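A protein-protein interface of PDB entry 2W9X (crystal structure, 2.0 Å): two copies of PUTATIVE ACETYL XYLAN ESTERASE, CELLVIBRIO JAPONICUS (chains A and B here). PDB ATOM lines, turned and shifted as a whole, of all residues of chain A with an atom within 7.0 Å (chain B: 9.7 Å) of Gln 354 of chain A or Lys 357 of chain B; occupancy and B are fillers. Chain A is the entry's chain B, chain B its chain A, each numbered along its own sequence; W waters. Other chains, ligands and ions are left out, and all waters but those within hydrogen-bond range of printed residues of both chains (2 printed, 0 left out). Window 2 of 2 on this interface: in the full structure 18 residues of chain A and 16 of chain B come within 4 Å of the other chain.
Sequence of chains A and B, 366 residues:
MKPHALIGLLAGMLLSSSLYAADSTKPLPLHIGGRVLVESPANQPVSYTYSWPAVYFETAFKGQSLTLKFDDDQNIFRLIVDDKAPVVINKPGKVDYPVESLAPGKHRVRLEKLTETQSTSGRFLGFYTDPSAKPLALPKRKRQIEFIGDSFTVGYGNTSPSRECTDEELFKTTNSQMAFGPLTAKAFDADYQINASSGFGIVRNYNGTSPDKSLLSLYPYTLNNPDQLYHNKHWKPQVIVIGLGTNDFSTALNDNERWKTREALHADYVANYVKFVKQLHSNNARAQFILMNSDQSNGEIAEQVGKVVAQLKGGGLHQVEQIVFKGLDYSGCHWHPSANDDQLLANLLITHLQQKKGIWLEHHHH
The backbone carbonyl oxygen (O) of Gln 354 of chain A lies within hydrogen-bond range of the side-chain amino group (NZ) of Lys 357 of chain B, 2.9 Å away.
O of Gln 355 of chain B is in hydrogen-bond range of N of Lys 357 of chain A (2.7 Å).
The backbone carbonyl oxygen (O) of Gln 355 of chain B lies close to the backbone carbonyl oxygen (O) of Gln 355 of chain A (3.4 Å).
N of Lys 357 of chain B sits at hydrogen-bond distance from O of Gln 355 of chain A (2.7 Å).
OE2 of Glu 321 of chain B lies within salt-bridge range of NZ of Lys 356 of chain B, at 3.2 Å.
Among the printed residues, merely in contact across the chains: Gln 355 of chain A with Lys 356 of chain B (3.5 Å), Lys 356 of chain A with Gln 355 of chain B (3.6 Å), Lys 357 of chain A with Gln 354 of chain B (3.3 Å) and Lys 357 of chain A with Lys 357 of chain B (3.6 Å).
No residue of chain B comes within 4 Å of Thr 351 of chain A.
Of chain B, only Lys 357 (2.9 Å) comes within 4 Å of Gln 354 of chain A.
Of the printed residues of chain B, Lys 356 of chain A touches Gln 355.
Ile 359 of chain A touches none of the printed residues of chain B.
Printed residues of chain A within 4 Å of Gln 354 of chain B: Lys 357 (3.3 Å).
Printed residues of chain A within 4 Å of Lys 356 of chain B: Gln 355.
Lys 357 of chain B touches just these residues of chain A: Gln 354 (2.9 Å), Gln 355 (2.7 Å) and Lys 357 (3.6 Å).
The nearest residue of chain B that does not touch Gln 354 of chain A is Gln 355 of chain B (6.9 Å).
The nearest printed residue of chain A that does not touch Gln 355 of chain B is Gly 358 of chain A (4.6 Å).
Of the 14 printed residues of chain B, 4 touch a printed residue of chain A.
Printed residues of chain B that touch a printed residue of chain A: Gln 354, Gln 355, Lys 356 and Lys 357.
Printed residues of chain A that touch a printed residue of chain B: Gln 354, Gln 355, Lys 356 and Lys 357.
Among the printed residues, no Asp or Glu carboxylate lies within 4 Å of a Lys or Arg side-chain nitrogen of the other chain.
Gln 354 of chain A touches Lys 357 of chain B, and with the chains exchanged Lys 357 of chain A touches Gln 354 of chain B.
Gln 355 of chain B touches its own counterpart, Gln 355 of chain A.
Gln 355 of chain A touches Lys 356 of chain B, and with the chains exchanged Lys 356 of chain A touches Gln 355 of chain B.
Lys 357 of chain A touches its own counterpart, Lys 357 of chain B.
Positions printed for both chains: 351, 352, 353, 354, 355, 356, 357, 358, 359 and 360.
Of the 8 pairs that touch across the chains among the printed residues, 8 have their exchanged pair printed and touching as well.
Water W2 lies within hydrogen-bond range of the backbone carbonyl oxygen (O) of Lys 356 of chain B (3.0 Å), the backbone carbonyl oxygen (O) of Leu 353 of chain B (3.1 Å) and the side-chain amino group (NZ) of Lys 357 of chain A (3.4 Å).
Water W1 lies within hydrogen-bond range of the side-chain amino group (NZ) of Lys 356 of chain A and the side-chain amino group (NZ) of Lys 356 of chain B.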
ATOM      1  N   ALA A 187     -15.075 -13.818   7.262  1.00  0.00           N
ATOM      2  CA  ALA A 187     -14.431 -12.563   6.841  1.00  0.00           C
ATOM      3  C   ALA A 187     -14.561 -11.469   7.907  1.00  0.00           C
ATOM      4  O   ALA A 187     -13.765 -10.529   7.941  1.00  0.00           O
ATOM      5  CB  ALA A 187     -14.986 -12.079   5.496  1.00  0.00           C
ATOM      6  N   PHE A 188     -15.558 -11.599   8.781  1.00  0.00           N
ATOM      7  CA  PHE A 188     -15.780 -10.620   9.842  1.00  0.00           C
ATOM      8  C   PHE A 188     -15.462 -11.181  11.237  1.00  0.00           C
ATOM      9  O   PHE A 188     -15.665 -10.494  12.235  1.00  0.00           O
ATOM     10  CB  PHE A 188     -17.225 -10.096   9.796  1.00  0.00           C
ATOM     11  CG  PHE A 188     -17.552  -9.308   8.556  1.00  0.00           C
ATOM     12  CD1 PHE A 188     -17.171  -7.970   8.442  1.00  0.00           C
ATOM     13  CD2 PHE A 188     -18.256  -9.898   7.499  1.00  0.00           C
ATOM     14  CE1 PHE A 188     -17.468  -7.224   7.280  1.00  0.00           C
ATOM     15  CE2 PHE A 188     -18.560  -9.164   6.332  1.00  0.00           C
ATOM     16  CZ  PHE A 188     -18.170  -7.824   6.223  1.00  0.00           C
ATOM     17  N   ASN A 347     -18.561 -12.794  -1.424  1.00  0.00           N
ATOM     18  CA  ASN A 347     -17.901 -11.521  -1.745  1.00  0.00           C
ATOM     19  C   ASN A 347     -18.907 -10.406  -1.871  1.00  0.00           C
ATOM     20  O   ASN A 347     -18.652  -9.287  -1.434  1.00  0.00           O
ATOM     21  CB  ASN A 347     -17.058 -11.624  -3.034  1.00  0.00           C
ATOM     22  CG  ASN A 347     -15.953 -12.654  -2.935  1.00  0.00           C
ATOM     23  OD1 ASN A 347     -15.545 -13.044  -1.837  1.00  0.00           O
ATOM     24  ND2 ASN A 347     -15.466 -13.112  -4.086  1.00  0.00           N
ATOM     25  N   LEU A 349     -21.858 -10.218  -0.315  1.00  0.00           N
ATOM     26  CA  LEU A 349     -22.298  -9.947   1.056  1.00  0.00           C
ATOM     27  C   LEU A 349     -21.229  -9.216   1.881  1.00  0.00           C
ATOM     28  O   LEU A 349     -21.526  -8.238   2.579  1.00  0.00           O
ATOM     29  CB  LEU A 349     -22.681 -11.271   1.721  1.00  0.00           C
ATOM     30  CG  LEU A 349     -24.039 -11.879   1.350  1.00  0.00           C
ATOM     31  CD1 LEU A 349     -24.119 -13.282   1.885  1.00  0.00           C
ATOM     32  CD2 LEU A 349     -25.168 -11.032   1.934  1.00  0.00           C
ATOM     33  N   ILE A 350     -19.987  -9.694   1.794  1.00  0.00           N
ATOM     34  CA  ILE A 350     -18.861  -9.061   2.498  1.00  0.00           C
ATOM     35  C   ILE A 350     -18.713  -7.574   2.157  1.00  0.00           C
ATOM     36  O   ILE A 350     -18.635  -6.723   3.057  1.00  0.00           O
ATOM     37  CB  ILE A 350     -17.540  -9.822   2.246  1.00  0.00           C
ATOM     38  CG1 ILE A 350     -17.607 -11.205   2.891  1.00  0.00           C
ATOM     39  CG2 ILE A 350     -16.307  -8.983   2.717  1.00  0.00           C
ATOM     40  CD1 ILE A 350     -16.629 -12.249   2.314  1.00  0.00           C
ATOM     41  N   THR A 351     -18.697  -7.266   0.862  1.00  0.00           N
ATOM     42  CA  THR A 351     -18.623  -5.893   0.373  1.00  0.00           C
ATOM     43  C   THR A 351     -19.808  -5.050   0.847  1.00  0.00           C
ATOM     44  O   THR A 351     -19.638  -3.897   1.248  1.00  0.00           O
ATOM     45  CB  THR A 351     -18.540  -5.871  -1.179  1.00  0.00           C
ATOM     46  OG1 THR A 351     -17.489  -6.750  -1.603  1.00  0.00           O
ATOM     47  CG2 THR A 351     -18.267  -4.468  -1.713  1.00  0.00           C
ATOM     48  N   HIS A 352     -21.009  -5.629   0.784  1.00  0.00           N
ATOM     49  CA  HIS A 352     -22.222  -4.962   1.251  1.00  0.00           C
ATOM     50  C   HIS A 352     -22.070  -4.613   2.732  1.00  0.00           C
ATOM     51  O   HIS A 352     -22.293  -3.474   3.123  1.00  0.00           O
ATOM     52  CB  HIS A 352     -23.450  -5.857   1.032  1.00  0.00           C
ATOM     53  CG  HIS A 352     -24.744  -5.208   1.405  1.00  0.00           C
ATOM     54  ND1 HIS A 352     -25.450  -4.402   0.537  1.00  0.00           N
ATOM     55  CD2 HIS A 352     -25.457  -5.237   2.555  1.00  0.00           C
ATOM     56  CE1 HIS A 352     -26.541  -3.960   1.135  1.00  0.00           C
ATOM     57  NE2 HIS A 352     -26.571  -4.452   2.360  1.00  0.00           N
ATOM     58  N   LEU A 353     -21.675  -5.596   3.539  1.00  0.00           N
ATOM     59  CA  LEU A 353     -21.595  -5.409   4.993  1.00  0.00           C
ATOM     60  C   LEU A 353     -20.455  -4.466   5.416  1.00  0.00           C
ATOM     61  O   LEU A 353     -20.569  -3.779   6.430  1.00  0.00           O
ATOM     62  CB  LEU A 353     -21.524  -6.750   5.712  1.00  0.00           C
ATOM     63  CG  LEU A 353     -22.838  -7.520   5.601  1.00  0.00           C
ATOM     64  CD1 LEU A 353     -22.691  -8.936   6.117  1.00  0.00           C
ATOM     65  CD2 LEU A 353     -23.950  -6.780   6.341  1.00  0.00           C
ATOM     66  N   GLN A 354     -19.394  -4.417   4.609  1.00  0.00           N
ATOM     67  CA  GLN A 354     -18.264  -3.520   4.820  1.00  0.00           C
ATOM     68  C   GLN A 354     -18.641  -2.055   4.677  1.00  0.00           C
ATOM     69  O   GLN A 354     -17.995  -1.200   5.264  1.00  0.00           O
ATOM     70  CB  GLN A 354     -17.117  -3.845   3.844  1.00  0.00           C
ATOM     71  CG  GLN A 354     -16.228  -5.008   4.304  1.00  0.00           C
ATOM     72  CD  GLN A 354     -15.175  -5.428   3.266  1.00  0.00           C
ATOM     73  OE1 GLN A 354     -15.184  -4.973   2.114  1.00  0.00           O
ATOM     74  NE2 GLN A 354     -14.278  -6.316   3.673  1.00  0.00           N
ATOM     75  N   GLN A 355     -19.676  -1.761   3.896  1.00  0.00           N
ATOM     76  CA  GLN A 355     -20.040  -0.378   3.620  1.00  0.00           C
ATOM     77  C   GLN A 355     -21.007   0.190   4.657  1.00  0.00           C
ATOM     78  O   GLN A 355     -21.387   1.350   4.571  1.00  0.00           O
ATOM     79  CB  GLN A 355     -20.610  -0.213   2.195  1.00  0.00           C
ATOM     80  CG  GLN A 355     -19.620  -0.515   1.032  1.00  0.00           C
ATOM     81  CD  GLN A 355     -18.226   0.093   1.230  1.00  0.00           C
ATOM     82  OE1 GLN A 355     -17.285  -0.605   1.614  1.00  0.00           O
ATOM     83  NE2 GLN A 355     -18.092   1.397   0.965  1.00  0.00           N
ATOM     84  N   LYS A 356     -21.375  -0.623   5.642  1.00  0.00           N
ATOM     85  CA  LYS A 356     -22.417  -0.261   6.604  1.00  0.00           C
ATOM     86  C   LYS A 356     -21.808   0.103   7.955  1.00  0.00           C
ATOM     87  O   LYS A 356     -21.449  -0.775   8.741  1.00  0.00           O
ATOM     88  CB  LYS A 356     -23.452  -1.394   6.746  1.00  0.00           C
ATOM     89  CG  LYS A 356     -24.266  -1.678   5.465  1.00  0.00           C
ATOM     90  CD  LYS A 356     -25.440  -2.638   5.712  1.00  0.00           C
ATOM     91  CE  LYS A 356     -26.633  -1.964   6.444  1.00  0.00           C
ATOM     92  NZ  LYS A 356     -27.295  -0.854   5.693  1.00  0.00           N
ATOM     93  N   LYS A 357     -21.682   1.403   8.209  1.00  0.00           N
ATOM     94  CA  LYS A 357     -21.118   1.902   9.469  1.00  0.00           C
ATOM     95  C   LYS A 357     -21.917   1.437  10.676  1.00  0.00           C
ATOM     96  O   LYS A 357     -23.130   1.662  10.752  1.00  0.00           O
ATOM     97  CB  LYS A 357     -21.008   3.433   9.462  1.00  0.00           C
ATOM     98  CG  LYS A 357     -19.649   3.935   9.016  1.00  0.00           C
ATOM     99  CD  LYS A 357     -19.748   5.151   8.102  1.00  0.00           C
ATOM    100  CE  LYS A 357     -19.356   6.433   8.798  1.00  0.00           C
ATOM    101  NZ  LYS A 357     -19.053   7.463   7.754  1.00  0.00           N
ATOM    102  N   GLY A 358     -21.226   0.762  11.594  1.00  0.00           N
ATOM    103  CA  GLY A 358     -21.790   0.367  12.885  1.00  0.00           C
ATOM    104  C   GLY A 358     -22.824  -0.741  12.828  1.00  0.00           C
ATOM    105  O   GLY A 358     -23.640  -0.888  13.748  1.00  0.00           O
ATOM    106  N   ILE A 359     -22.778  -1.537  11.761  1.00  0.00           N
ATOM    107  CA  ILE A 359     -23.689  -2.669  11.612  1.00  0.00           C
ATOM    108  C   ILE A 359     -23.502  -3.728  12.702  1.00  0.00           C
ATOM    109  O   ILE A 359     -24.424  -4.481  12.990  1.00  0.00           O
ATOM    110  CB  ILE A 359     -23.623  -3.303  10.191  1.00  0.00           C
ATOM    111  CG1 ILE A 359     -24.847  -4.197   9.975  1.00  0.00           C
ATOM    112  CG2 ILE A 359     -22.313  -4.068   9.973  1.00  0.00           C
ATOM    113  CD1 ILE A 359     -25.253  -4.362   8.557  1.00  0.00           C
ATOM    114  N   TRP A 360     -22.312  -3.782  13.298  1.00  0.00           N
ATOM    115  CA  TRP A 360     -22.051  -4.697  14.408  1.00  0.00           C
ATOM    116  C   TRP A 360     -22.346  -4.062  15.782  1.00  0.00           C
ATOM    117  O   TRP A 360     -22.184  -4.710  16.812  1.00  0.00           O
ATOM    118  CB  TRP A 360     -20.622  -5.260  14.338  1.00  0.00           C
ATOM    119  CG  TRP A 360     -20.292  -5.884  13.011  1.00  0.00           C
ATOM    120  CD1 TRP A 360     -19.413  -5.406  12.077  1.00  0.00           C
ATOM    121  CD2 TRP A 360     -20.859  -7.078  12.455  1.00  0.00           C
ATOM    122  NE1 TRP A 360     -19.389  -6.237  10.977  1.00  0.00           N
ATOM    123  CE2 TRP A 360     -20.269  -7.268  11.181  1.00  0.00           C
ATOM    124  CE3 TRP A 360     -21.812  -8.004  12.903  1.00  0.00           C
ATOM    125  CZ2 TRP A 360     -20.600  -8.349  10.351  1.00  0.00           C
ATOM    126  CZ3 TRP A 360     -22.132  -9.086  12.084  1.00  0.00           C
ATOM    127  CH2 TRP A 360     -21.526  -9.246  10.822  1.00  0.00           C
ATOM    128  N   VAL B 239     -24.969  11.059  -4.712  1.00  0.00           N
ATOM    129  CA  VAL B 239     -26.273  10.638  -4.159  1.00  0.00           C
ATOM    130  C   VAL B 239     -27.439  11.283  -4.924  1.00  0.00           C
ATOM    131  O   VAL B 239     -27.453  12.499  -5.124  1.00  0.00           O
ATOM    132  CB  VAL B 239     -26.399  10.988  -2.648  1.00  0.00           C
ATOM    133  CG1 VAL B 239     -27.692  10.419  -2.084  1.00  0.00           C
ATOM    134  CG2 VAL B 239     -25.221  10.439  -1.859  1.00  0.00           C
ATOM    135  N   GLN B 288     -25.517   6.930  -6.328  1.00  0.00           N
ATOM    136  CA  GLN B 288     -26.273   5.963  -5.553  1.00  0.00           C
ATOM    137  C   GLN B 288     -27.656   6.540  -5.290  1.00  0.00           C
ATOM    138  O   GLN B 288     -27.790   7.721  -4.955  1.00  0.00           O
ATOM    139  CB  GLN B 288     -25.522   5.566  -4.276  1.00  0.00           C
ATOM    140  CG  GLN B 288     -24.124   5.000  -4.600  1.00  0.00           C
ATOM    141  CD  GLN B 288     -23.497   4.220  -3.464  1.00  0.00           C
ATOM    142  OE1 GLN B 288     -24.103   3.288  -2.912  1.00  0.00           O
ATOM    143  NE2 GLN B 288     -22.260   4.582  -3.119  1.00  0.00           N
ATOM    144  N   GLU B 321     -31.878   1.967  -3.098  1.00  0.00           N
ATOM    145  CA  GLU B 321     -32.565   1.640  -1.855  1.00  0.00           C
ATOM    146  C   GLU B 321     -33.894   2.384  -1.788  1.00  0.00           C
ATOM    147  O   GLU B 321     -34.089   3.424  -2.448  1.00  0.00           O
ATOM    148  CB  GLU B 321     -31.746   2.076  -0.641  1.00  0.00           C
ATOM    149  CG  GLU B 321     -30.325   1.563  -0.554  1.00  0.00           C
ATOM    150  CD  GLU B 321     -29.579   2.222   0.598  1.00  0.00           C
ATOM    151  OE1 GLU B 321     -29.539   1.630   1.699  1.00  0.00           O
ATOM    152  OE2 GLU B 321     -29.073   3.354   0.405  1.00  0.00           O
ATOM    153  N   THR B 351     -29.198  10.590   8.841  1.00  0.00           N
ATOM    154  CA  THR B 351     -28.822   9.397   9.584  1.00  0.00           C
ATOM    155  C   THR B 351     -28.516   8.215   8.647  1.00  0.00           C
ATOM    156  O   THR B 351     -27.582   7.437   8.891  1.00  0.00           O
ATOM    157  CB  THR B 351     -29.924   9.053  10.608  1.00  0.00           C
ATOM    158  OG1 THR B 351     -30.046  10.157  11.517  1.00  0.00           O
ATOM    159  CG2 THR B 351     -29.590   7.797  11.392  1.00  0.00           C
ATOM    160  N   HIS B 352     -29.311   8.102   7.582  1.00  0.00           N
ATOM    161  CA  HIS B 352     -29.172   7.048   6.589  1.00  0.00           C
ATOM    162  C   HIS B 352     -27.834   7.165   5.850  1.00  0.00           C
ATOM    163  O   HIS B 352     -27.098   6.191   5.741  1.00  0.00           O
ATOM    164  CB  HIS B 352     -30.326   7.134   5.585  1.00  0.00           C
ATOM    165  CG  HIS B 352     -30.266   6.101   4.502  1.00  0.00           C
ATOM    166  ND1 HIS B 352     -30.902   4.881   4.601  1.00  0.00           N
ATOM    167  CD2 HIS B 352     -29.648   6.107   3.297  1.00  0.00           C
ATOM    168  CE1 HIS B 352     -30.682   4.180   3.501  1.00  0.00           C
ATOM    169  NE2 HIS B 352     -29.919   4.898   2.697  1.00  0.00           N
ATOM    170  N   LEU B 353     -27.539   8.363   5.348  1.00  0.00           N
ATOM    171  CA  LEU B 353     -26.293   8.609   4.602  1.00  0.00           C
ATOM    172  C   LEU B 353     -25.042   8.580   5.477  1.00  0.00           C
ATOM    173  O   LEU B 353     -23.965   8.214   5.002  1.00  0.00           O
ATOM    174  CB  LEU B 353     -26.380   9.916   3.821  1.00  0.00           C
ATOM    175  CG  LEU B 353     -27.432   9.946   2.716  1.00  0.00           C
ATOM    176  CD1 LEU B 353     -27.774  11.370   2.331  1.00  0.00           C
ATOM    177  CD2 LEU B 353     -26.998   9.131   1.487  1.00  0.00           C
ATOM    178  N   GLN B 354     -25.191   8.919   6.758  1.00  0.00           N
ATOM    179  CA  GLN B 354     -24.077   8.862   7.710  1.00  0.00           C
ATOM    180  C   GLN B 354     -23.614   7.437   8.013  1.00  0.00           C
ATOM    181  O   GLN B 354     -22.495   7.236   8.472  1.00  0.00           O
ATOM    182  CB  GLN B 354     -24.443   9.572   9.024  1.00  0.00           C
ATOM    183  CG  GLN B 354     -24.587  11.093   8.908  1.00  0.00           C
ATOM    184  CD  GLN B 354     -24.905  11.775  10.239  1.00  0.00           C
ATOM    185  OE1 GLN B 354     -25.224  11.121  11.238  1.00  0.00           O
ATOM    186  NE2 GLN B 354     -24.831  13.101  10.246  1.00  0.00           N
ATOM    187  N   GLN B 355     -24.484   6.451   7.782  1.00  0.00           N
ATOM    188  CA  GLN B 355     -24.125   5.044   8.002  1.00  0.00           C
ATOM    189  C   GLN B 355     -23.504   4.390   6.759  1.00  0.00           C
ATOM    190  O   GLN B 355     -23.042   3.265   6.823  1.00  0.00           O
ATOM    191  CB  GLN B 355     -25.339   4.217   8.462  1.00  0.00           C
ATOM    192  CG  GLN B 355     -26.067   4.731   9.704  1.00  0.00           C
ATOM    193  CD  GLN B 355     -25.132   5.091  10.866  1.00  0.00           C
ATOM    194  OE1 GLN B 355     -25.098   6.248  11.303  1.00  0.00           O
ATOM    195  NE2 GLN B 355     -24.370   4.108  11.363  1.00  0.00           N
ATOM    196  N   LYS B 356     -23.498   5.092   5.634  1.00  0.00           N
ATOM    197  CA  LYS B 356     -22.943   4.532   4.405  1.00  0.00           C
ATOM    198  C   LYS B 356     -21.456   4.900   4.193  1.00  0.00           C
ATOM    199  O   LYS B 356     -21.145   6.019   3.792  1.00  0.00           O
ATOM    200  CB  LYS B 356     -23.798   4.948   3.199  1.00  0.00           C
ATOM    201  CG  LYS B 356     -25.266   4.506   3.273  1.00  0.00           C
ATOM    202  CD  LYS B 356     -26.054   4.822   1.986  1.00  0.00           C
ATOM    203  CE  LYS B 356     -25.727   3.861   0.814  1.00  0.00           C
ATOM    204  NZ  LYS B 356     -26.131   2.423   1.058  1.00  0.00           N
ATOM    205  N   LYS B 357     -20.551   3.956   4.463  1.00  0.00           N
ATOM    206  CA  LYS B 357     -19.107   4.161   4.248  1.00  0.00           C
ATOM    207  C   LYS B 357     -18.765   4.518   2.806  1.00  0.00           C
ATOM    208  O   LYS B 357     -19.258   3.891   1.869  1.00  0.00           O
ATOM    209  CB  LYS B 357     -18.308   2.913   4.623  1.00  0.00           C
ATOM    210  CG  LYS B 357     -18.007   2.755   6.083  1.00  0.00           C
ATOM    211  CD  LYS B 357     -17.034   1.611   6.311  1.00  0.00           C
ATOM    212  CE  LYS B 357     -17.306   0.925   7.652  1.00  0.00           C
ATOM    213  NZ  LYS B 357     -16.618  -0.396   7.729  1.00  0.00           N
ATOM    214  N   GLY B 358     -17.917   5.528   2.638  1.00  0.00           N
ATOM    215  CA  GLY B 358     -17.416   5.932   1.323  1.00  0.00           C
ATOM    216  C   GLY B 358     -18.464   6.399   0.329  1.00  0.00           C
ATOM    217  O   GLY B 358     -18.219   6.392  -0.872  1.00  0.00           O
ATOM    218  N   ILE B 359     -19.627   6.812   0.836  1.00  0.00           N
ATOM    219  CA  ILE B 359     -20.736   7.294   0.002  1.00  0.00           C
ATOM    220  C   ILE B 359     -20.400   8.555  -0.807  1.00  0.00           C
ATOM    221  O   ILE B 359     -21.011   8.815  -1.853  1.00  0.00           O
ATOM    222  CB  ILE B 359     -22.047   7.520   0.852  1.00  0.00           C
ATOM    223  CG1 ILE B 359     -23.274   7.675  -0.048  1.00  0.00           C
ATOM    224  CG2 ILE B 359     -21.919   8.703   1.809  1.00  0.00           C
ATOM    225  CD1 ILE B 359     -23.712   6.383  -0.680  1.00  0.00           C
ATOM    226  N   TRP B 360     -19.438   9.336  -0.319  1.00  0.00           N
ATOM    227  CA  TRP B 360     -19.039  10.570  -1.000  1.00  0.00           C
ATOM    228  C   TRP B 360     -17.802  10.408  -1.878  1.00  0.00           C
ATOM    229  O   TRP B 360     -17.580  11.212  -2.785  1.00  0.00           O
ATOM    230  CB  TRP B 360     -18.836  11.711  -0.003  1.00  0.00           C
ATOM    231  CG  TRP B 360     -20.052  11.996   0.801  1.00  0.00           C
ATOM    232  CD1 TRP B 360     -20.215  11.777   2.136  1.00  0.00           C
ATOM    233  CD2 TRP B 360     -21.295  12.527   0.323  1.00  0.00           C
ATOM    234  NE1 TRP B 360     -21.479  12.148   2.523  1.00  0.00           N
ATOM    235  CE2 TRP B 360     -22.163  12.613   1.431  1.00  0.00           C
ATOM    236  CE3 TRP B 360     -21.759  12.941  -0.934  1.00  0.00           C
ATOM    237  CZ2 TRP B 360     -23.465  13.104   1.327  1.00  0.00           C
ATOM    238  CZ3 TRP B 360     -23.054  13.431  -1.040  1.00  0.00           C
ATOM    239  CH2 TRP B 360     -23.895  13.504   0.089  1.00  0.00           C
ATOM    240  N   LEU B 361     -17.009   9.372  -1.612  1.00  0.00           N
ATOM    241  CA  LEU B 361     -15.793   9.120  -2.380  1.00  0.00           C
ATOM    242  C   LEU B 361     -16.091   8.429  -3.707  1.00  0.00           C
ATOM    243  O   LEU B 361     -16.887   8.926  -4.511  1.00  0.00           O
ATOM    244  CB  LEU B 361     -14.793   8.305  -1.553  1.00  0.00           C
ATOM    245  CG  LEU B 361     -13.951   9.036  -0.488  1.00  0.00           C
ATOM    246  CD1 LEU B 361     -13.341  10.355  -1.032  1.00  0.00           C
ATOM    247  CD2 LEU B 361     -14.727   9.261   0.825  1.00  0.00           C
HETATM  248  O   HOH W   1     -26.551  -0.523   2.759  1.00  0.00           O
HETATM  249  O   HOH W   2     -20.952   8.656   5.206  1.00  0.00           O
